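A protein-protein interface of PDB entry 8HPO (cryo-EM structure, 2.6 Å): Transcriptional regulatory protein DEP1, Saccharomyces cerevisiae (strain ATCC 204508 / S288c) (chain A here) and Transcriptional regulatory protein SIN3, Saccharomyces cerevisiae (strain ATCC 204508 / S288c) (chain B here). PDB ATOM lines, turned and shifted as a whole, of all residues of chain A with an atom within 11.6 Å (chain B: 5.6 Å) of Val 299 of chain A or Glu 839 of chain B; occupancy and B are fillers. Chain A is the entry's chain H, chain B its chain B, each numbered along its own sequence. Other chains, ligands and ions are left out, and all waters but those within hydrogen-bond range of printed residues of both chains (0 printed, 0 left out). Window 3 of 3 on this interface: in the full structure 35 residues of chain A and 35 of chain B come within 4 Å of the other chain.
Asp 297 of chain A touches Asn 836 of chain B (O to OD1, 3.8 Å).
Val 835 of chain B touches Val 299 of chain A.
Val 299 of chain A touches Glu 839 of chain B (CG2 to OE1, 3.9 Å).
Ile 300 of chain A touches Pro 892 of chain B (CD1 to O, 3.4 Å).
CD1 of Ile 300 of chain A touches CD2 of Leu 895 of chain B, 3.6 Å away.
Of chain B, only Val 835 and Glu 839 come within 4 Å of Val 299 of chain A.
Of the printed residues of chain A, Glu 839 of chain B touches Val 299.
Val 835 of chain B touches one residue of chain A.
No residue of chain A comes within 4 Å of Ile 838 of chain B.
Met 841 of chain B touches none of the printed residues of chain A.
Of chain A, only Ile 300 comes within 4 Å of Pro 892 of chain B.
Printed residues of chain A within 4 Å of Leu 895 of chain B: Ile 300.
Of the printed residues of chain B, Asp 297 of chain A touches Asn 836 (3.8 Å).
Of the printed residues of chain B, Ile 300 of chain A touches Pro 892 (3.4 Å) and Leu 895 (3.6 Å).
Arg 294 of chain A touches none of the printed residues of chain B.
Lys 837 of chain B touches none of the printed residues of chain A.
The nearest residue of chain B that does not touch Val 299 of chain A is Asn 836 of chain B (4.4 Å).
The nearest printed residue of chain B that does not touch Asp 297 of chain A is Asn 840 of chain B (5.1 Å).
Of the 11 printed residues of chain A, 3 touch a printed residue of chain B.
Hydrophobic or aromatic side chains of chain A within 4 Å of the printed part of chain B: Val 299 and Ile 300.
Along chain A the printed residues that touch a printed residue of chain B span positions 297 to 300.
Of the 11 printed residues of chain B, 5 touch a printed residue of chain A.
Printed residues of chain B that touch a printed residue of chain A: Val 835, Asn 836, Glu 839, Pro 892 and Leu 895.
Hydrophobic or aromatic side chains of chain B that line the printed part of chain A: Val 835, Pro 892 and Leu 895.
Along chain B the printed residues that touch a printed residue of chain A span positions 835 to 895.
Among the printed residues, no Asp or Glu carboxylate lies within 4 Å of a Lys or Arg side-chain nitrogen of the other chain.
The side-chain amide oxygen (OD1) of Asn 840 of chain B sits close to the backbone carbonyl oxygen (O) of Asn 836 of chain B (3.3 Å).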
ATOM      1  N   ARG A 293      11.194 -10.815  -4.330  1.00  0.00           N
ATOM      2  CA  ARG A 293      11.555  -9.510  -3.792  1.00  0.00           C
ATOM      3  C   ARG A 293      10.514  -9.036  -2.795  1.00  0.00           C
ATOM      4  O   ARG A 293      10.847  -8.658  -1.665  1.00  0.00           O
ATOM      5  CB  ARG A 293      11.701  -8.493  -4.919  1.00  0.00           C
ATOM      6  CG  ARG A 293      11.871  -7.072  -4.430  1.00  0.00           C
ATOM      7  CD  ARG A 293      13.211  -6.897  -3.730  1.00  0.00           C
ATOM      8  NE  ARG A 293      13.103  -6.043  -2.553  1.00  0.00           N
ATOM      9  CZ  ARG A 293      13.080  -4.717  -2.592  1.00  0.00           C
ATOM     10  NH1 ARG A 293      13.165  -4.082  -3.751  1.00  0.00           N
ATOM     11  NH2 ARG A 293      12.972  -4.025  -1.469  1.00  0.00           N
ATOM     12  N   ARG A 294       9.243  -9.046  -3.195  1.00  0.00           N
ATOM     13  CA  ARG A 294       8.205  -8.569  -2.286  1.00  0.00           C
ATOM     14  C   ARG A 294       8.080  -9.442  -1.045  1.00  0.00           C
ATOM     15  O   ARG A 294       7.675  -8.950   0.012  1.00  0.00           O
ATOM     16  CB  ARG A 294       6.863  -8.480  -3.001  1.00  0.00           C
ATOM     17  CG  ARG A 294       6.819  -7.419  -4.072  1.00  0.00           C
ATOM     18  CD  ARG A 294       5.411  -7.257  -4.600  1.00  0.00           C
ATOM     19  NE  ARG A 294       4.582  -8.415  -4.286  1.00  0.00           N
ATOM     20  CZ  ARG A 294       4.453  -9.479  -5.072  1.00  0.00           C
ATOM     21  NH1 ARG A 294       5.104  -9.540  -6.225  1.00  0.00           N
ATOM     22  NH2 ARG A 294       3.675 -10.487  -4.700  1.00  0.00           N
ATOM     23  N   ASP A 295       8.420 -10.726  -1.138  1.00  0.00           N
ATOM     24  CA  ASP A 295       8.349 -11.586   0.037  1.00  0.00           C
ATOM     25  C   ASP A 295       9.381 -11.240   1.102  1.00  0.00           C
ATOM     26  O   ASP A 295       9.251 -11.708   2.236  1.00  0.00           O
ATOM     27  CB  ASP A 295       8.507 -13.051  -0.364  1.00  0.00           C
ATOM     28  CG  ASP A 295       7.235 -13.639  -0.939  1.00  0.00           C
ATOM     29  OD1 ASP A 295       6.301 -12.865  -1.231  1.00  0.00           O
ATOM     30  OD2 ASP A 295       7.169 -14.876  -1.097  1.00  0.00           O
ATOM     31  N   MET A 296      10.401 -10.451   0.773  1.00  0.00           N
ATOM     32  CA  MET A 296      11.353  -9.959   1.760  1.00  0.00           C
ATOM     33  C   MET A 296      10.890  -8.672   2.421  1.00  0.00           C
ATOM     34  O   MET A 296      11.597  -8.148   3.287  1.00  0.00           O
ATOM     35  CB  MET A 296      12.727  -9.727   1.117  1.00  0.00           C
ATOM     36  CG  MET A 296      13.509 -10.994   0.827  1.00  0.00           C
ATOM     37  SD  MET A 296      15.267 -10.676   0.597  1.00  0.00           S
ATOM     38  CE  MET A 296      15.206  -9.349  -0.599  1.00  0.00           C
ATOM     39  N   ASP A 297       9.729  -8.156   2.030  1.00  0.00           N
ATOM     40  CA  ASP A 297       9.180  -6.922   2.566  1.00  0.00           C
ATOM     41  C   ASP A 297       8.204  -7.154   3.710  1.00  0.00           C
ATOM     42  O   ASP A 297       7.774  -6.186   4.341  1.00  0.00           O
ATOM     43  CB  ASP A 297       8.487  -6.137   1.450  1.00  0.00           C
ATOM     44  CG  ASP A 297       8.644  -4.642   1.605  1.00  0.00           C
ATOM     45  OD1 ASP A 297       9.228  -4.008   0.703  1.00  0.00           O
ATOM     46  OD2 ASP A 297       8.177  -4.096   2.624  1.00  0.00           O
ATOM     47  N   ILE A 298       7.841  -8.407   3.993  1.00  0.00           N
ATOM     48  CA  ILE A 298       6.885  -8.678   5.056  1.00  0.00           C
ATOM     49  C   ILE A 298       7.578  -8.550   6.405  1.00  0.00           C
ATOM     50  O   ILE A 298       8.698  -9.041   6.604  1.00  0.00           O
ATOM     51  CB  ILE A 298       6.235 -10.063   4.872  1.00  0.00           C
ATOM     52  CG1 ILE A 298       7.255 -11.192   5.026  1.00  0.00           C
ATOM     53  CG2 ILE A 298       5.548 -10.153   3.524  1.00  0.00           C
ATOM     54  CD1 ILE A 298       7.254 -11.857   6.388  1.00  0.00           C
ATOM     55  N   VAL A 299       6.921  -7.858   7.332  1.00  0.00           N
ATOM     56  CA  VAL A 299       7.482  -7.588   8.649  1.00  0.00           C
ATOM     57  C   VAL A 299       6.804  -8.482   9.681  1.00  0.00           C
ATOM     58  O   VAL A 299       7.429  -8.908  10.658  1.00  0.00           O
ATOM     59  CB  VAL A 299       7.341  -6.095   8.992  1.00  0.00           C
ATOM     60  CG1 VAL A 299       5.958  -5.603   8.614  1.00  0.00           C
ATOM     61  CG2 VAL A 299       7.627  -5.839  10.460  1.00  0.00           C
ATOM     62  N   ILE A 300       5.532  -8.794   9.460  1.00  0.00           N
ATOM     63  CA  ILE A 300       4.762  -9.675  10.329  1.00  0.00           C
ATOM     64  C   ILE A 300       4.070 -10.705   9.449  1.00  0.00           C
ATOM     65  O   ILE A 300       3.193 -10.343   8.663  1.00  0.00           O
ATOM     66  CB  ILE A 300       3.727  -8.915  11.178  1.00  0.00           C
ATOM     67  CG1 ILE A 300       4.426  -8.119  12.274  1.00  0.00           C
ATOM     68  CG2 ILE A 300       2.728  -9.879  11.789  1.00  0.00           C
ATOM     69  CD1 ILE A 300       4.030  -6.681  12.302  1.00  0.00           C
ATOM     70  N   PRO A 301       4.427 -11.979   9.539  1.00  0.00           N
ATOM     71  CA  PRO A 301       3.800 -12.987   8.684  1.00  0.00           C
ATOM     72  C   PRO A 301       2.404 -13.351   9.164  1.00  0.00           C
ATOM     73  O   PRO A 301       1.903 -12.843  10.168  1.00  0.00           O
ATOM     74  CB  PRO A 301       4.748 -14.183   8.808  1.00  0.00           C
ATOM     75  CG  PRO A 301       5.363 -14.018  10.142  1.00  0.00           C
ATOM     76  CD  PRO A 301       5.527 -12.540  10.337  1.00  0.00           C
ATOM     77  N   ASP A 302       1.781 -14.260   8.422  1.00  0.00           N
ATOM     78  CA  ASP A 302       0.510 -14.822   8.847  1.00  0.00           C
ATOM     79  C   ASP A 302       0.731 -15.991   9.798  1.00  0.00           C
ATOM     80  O   ASP A 302       1.728 -16.712   9.716  1.00  0.00           O
ATOM     81  CB  ASP A 302      -0.299 -15.293   7.643  1.00  0.00           C
ATOM     82  CG  ASP A 302      -0.999 -14.161   6.940  1.00  0.00           C
ATOM     83  OD1 ASP A 302      -0.640 -12.995   7.190  1.00  0.00           O
ATOM     84  OD2 ASP A 302      -1.913 -14.434   6.137  1.00  0.00           O
ATOM     85  N   VAL A 303      -0.206 -16.170  10.707  1.00  0.00           N
ATOM     86  CA  VAL A 303      -0.248 -17.360  11.543  1.00  0.00           C
ATOM     87  C   VAL A 303      -1.352 -18.253  11.013  1.00  0.00           C
ATOM     88  O   VAL A 303      -2.318 -17.786  10.402  1.00  0.00           O
ATOM     89  CB  VAL A 303      -0.475 -17.018  13.028  1.00  0.00           C
ATOM     90  CG1 VAL A 303       0.722 -16.294  13.594  1.00  0.00           C
ATOM     91  CG2 VAL A 303      -1.716 -16.176  13.177  1.00  0.00           C
ATOM     92  N   ILE B 834       0.117   1.127   6.749  1.00  0.00           N
ATOM     93  CA  ILE B 834       0.865   2.012   7.641  1.00  0.00           C
ATOM     94  C   ILE B 834       2.182   1.366   8.074  1.00  0.00           C
ATOM     95  O   ILE B 834       3.245   1.997   8.024  1.00  0.00           O
ATOM     96  CB  ILE B 834       0.007   2.415   8.851  1.00  0.00           C
ATOM     97  CG1 ILE B 834      -0.840   3.640   8.522  1.00  0.00           C
ATOM     98  CG2 ILE B 834       0.884   2.708  10.049  1.00  0.00           C
ATOM     99  CD1 ILE B 834      -2.051   3.359   7.671  1.00  0.00           C
ATOM    100  N   VAL B 835       2.131   0.113   8.530  1.00  0.00           N
ATOM    101  CA  VAL B 835       3.331  -0.557   9.019  1.00  0.00           C
ATOM    102  C   VAL B 835       4.387  -0.625   7.929  1.00  0.00           C
ATOM    103  O   VAL B 835       5.592  -0.515   8.200  1.00  0.00           O
ATOM    104  CB  VAL B 835       2.976  -1.957   9.541  1.00  0.00           C
ATOM    105  CG1 VAL B 835       4.222  -2.735   9.863  1.00  0.00           C
ATOM    106  CG2 VAL B 835       2.124  -1.839  10.746  1.00  0.00           C
ATOM    107  N   ASN B 836       3.961  -0.794   6.677  1.00  0.00           N
ATOM    108  CA  ASN B 836       4.932  -0.823   5.590  1.00  0.00           C
ATOM    109  C   ASN B 836       5.548   0.550   5.372  1.00  0.00           C
ATOM    110  O   ASN B 836       6.744   0.658   5.082  1.00  0.00           O
ATOM    111  CB  ASN B 836       4.278  -1.347   4.315  1.00  0.00           C
ATOM    112  CG  ASN B 836       4.216  -2.855   4.285  1.00  0.00           C
ATOM    113  OD1 ASN B 836       5.059  -3.528   4.875  1.00  0.00           O
ATOM    114  ND2 ASN B 836       3.216  -3.396   3.602  1.00  0.00           N
ATOM    115  N   LYS B 837       4.752   1.613   5.513  1.00  0.00           N
ATOM    116  CA  LYS B 837       5.337   2.953   5.486  1.00  0.00           C
ATOM    117  C   LYS B 837       6.356   3.135   6.604  1.00  0.00           C
ATOM    118  O   LYS B 837       7.332   3.875   6.450  1.00  0.00           O
ATOM    119  CB  LYS B 837       4.251   4.015   5.606  1.00  0.00           C
ATOM    120  CG  LYS B 837       3.577   4.386   4.306  1.00  0.00           C
ATOM    121  CD  LYS B 837       2.814   5.696   4.453  1.00  0.00           C
ATOM    122  CE  LYS B 837       2.368   5.928   5.891  1.00  0.00           C
ATOM    123  NZ  LYS B 837       1.339   6.994   6.008  1.00  0.00           N
ATOM    124  N   ILE B 838       6.138   2.472   7.739  1.00  0.00           N
ATOM    125  CA  ILE B 838       6.960   2.741   8.919  1.00  0.00           C
ATOM    126  C   ILE B 838       8.256   1.940   8.889  1.00  0.00           C
ATOM    127  O   ILE B 838       9.280   2.390   9.415  1.00  0.00           O
ATOM    128  CB  ILE B 838       6.149   2.469  10.203  1.00  0.00           C
ATOM    129  CG1 ILE B 838       5.578   3.770  10.761  1.00  0.00           C
ATOM    130  CG2 ILE B 838       6.988   1.772  11.258  1.00  0.00           C
ATOM    131  CD1 ILE B 838       4.863   4.607   9.741  1.00  0.00           C
ATOM    132  N   GLU B 839       8.252   0.764   8.259  1.00  0.00           N
ATOM    133  CA  GLU B 839       9.431  -0.097   8.310  1.00  0.00           C
ATOM    134  C   GLU B 839      10.638   0.556   7.643  1.00  0.00           C
ATOM    135  O   GLU B 839      11.734   0.588   8.215  1.00  0.00           O
ATOM    136  CB  GLU B 839       9.130  -1.445   7.660  1.00  0.00           C
ATOM    137  CG  GLU B 839      10.364  -2.292   7.414  1.00  0.00           C
ATOM    138  CD  GLU B 839      10.932  -2.890   8.685  1.00  0.00           C
ATOM    139  OE1 GLU B 839      10.721  -4.096   8.918  1.00  0.00           O
ATOM    140  OE2 GLU B 839      11.591  -2.156   9.450  1.00  0.00           O
ATOM    141  N   ASN B 840      10.464   1.074   6.431  1.00  0.00           N
ATOM    142  CA  ASN B 840      11.583   1.644   5.677  1.00  0.00           C
ATOM    143  C   ASN B 840      11.681   3.138   5.965  1.00  0.00           C
ATOM    144  O   ASN B 840      11.125   3.974   5.255  1.00  0.00           O
ATOM    145  CB  ASN B 840      11.436   1.348   4.189  1.00  0.00           C
ATOM    146  CG  ASN B 840      10.029   1.583   3.671  1.00  0.00           C
ATOM    147  OD1 ASN B 840       9.328   2.497   4.103  1.00  0.00           O
ATOM    148  ND2 ASN B 840       9.607   0.747   2.729  1.00  0.00           N
ATOM    149  N   MET B 841      12.418   3.477   7.020  1.00  0.00           N
ATOM    150  CA  MET B 841      12.620   4.868   7.400  1.00  0.00           C
ATOM    151  C   MET B 841      14.009   5.007   8.008  1.00  0.00           C
ATOM    152  O   MET B 841      14.820   4.080   7.971  1.00  0.00           O
ATOM    153  CB  MET B 841      11.538   5.339   8.376  1.00  0.00           C
ATOM    154  CG  MET B 841      10.415   6.115   7.713  1.00  0.00           C
ATOM    155  SD  MET B 841       9.116   6.600   8.864  1.00  0.00           S
ATOM    156  CE  MET B 841       8.118   7.667   7.828  1.00  0.00           C
ATOM    157  N   LYS B 846      11.131   8.087  12.538  1.00  0.00           N
ATOM    158  CA  LYS B 846      10.206   7.250  13.292  1.00  0.00           C
ATOM    159  C   LYS B 846       9.721   7.966  14.544  1.00  0.00           C
ATOM    160  O   LYS B 846       8.514   8.152  14.738  1.00  0.00           O
ATOM    161  CB  LYS B 846      10.876   5.930  13.676  1.00  0.00           C
ATOM    162  CG  LYS B 846      11.139   4.976  12.534  1.00  0.00           C
ATOM    163  CD  LYS B 846      11.617   3.643  13.076  1.00  0.00           C
ATOM    164  CE  LYS B 846      12.068   2.716  11.964  1.00  0.00           C
ATOM    165  NZ  LYS B 846      12.628   1.440  12.490  1.00  0.00           N
ATOM    166  N   PRO B 892       3.326  -2.495  15.199  1.00  0.00           N
ATOM    167  CA  PRO B 892       3.559  -3.888  14.785  1.00  0.00           C
ATOM    168  C   PRO B 892       3.092  -4.903  15.815  1.00  0.00           C
ATOM    169  O   PRO B 892       3.188  -6.103  15.551  1.00  0.00           O
ATOM    170  CB  PRO B 892       5.084  -3.942  14.634  1.00  0.00           C
ATOM    171  CG  PRO B 892       5.587  -2.898  15.517  1.00  0.00           C
ATOM    172  CD  PRO B 892       4.603  -1.794  15.419  1.00  0.00           C
ATOM    173  N   LEU B 895      -0.981  -5.136  15.121  1.00  0.00           N
ATOM    174  CA  LEU B 895      -1.252  -5.845  13.877  1.00  0.00           C
ATOM    175  C   LEU B 895      -0.986  -7.335  13.997  1.00  0.00           C
ATOM    176  O   LEU B 895      -1.723  -8.138  13.422  1.00  0.00           O
ATOM    177  CB  LEU B 895      -0.418  -5.271  12.735  1.00  0.00           C
ATOM    178  CG  LEU B 895      -0.492  -6.097  11.452  1.00  0.00           C
ATOM    179  CD1 LEU B 895      -1.608  -5.604  10.550  1.00  0.00           C
ATOM    180  CD2 LEU B 895       0.836  -6.095  10.732  1.00  0.00           C
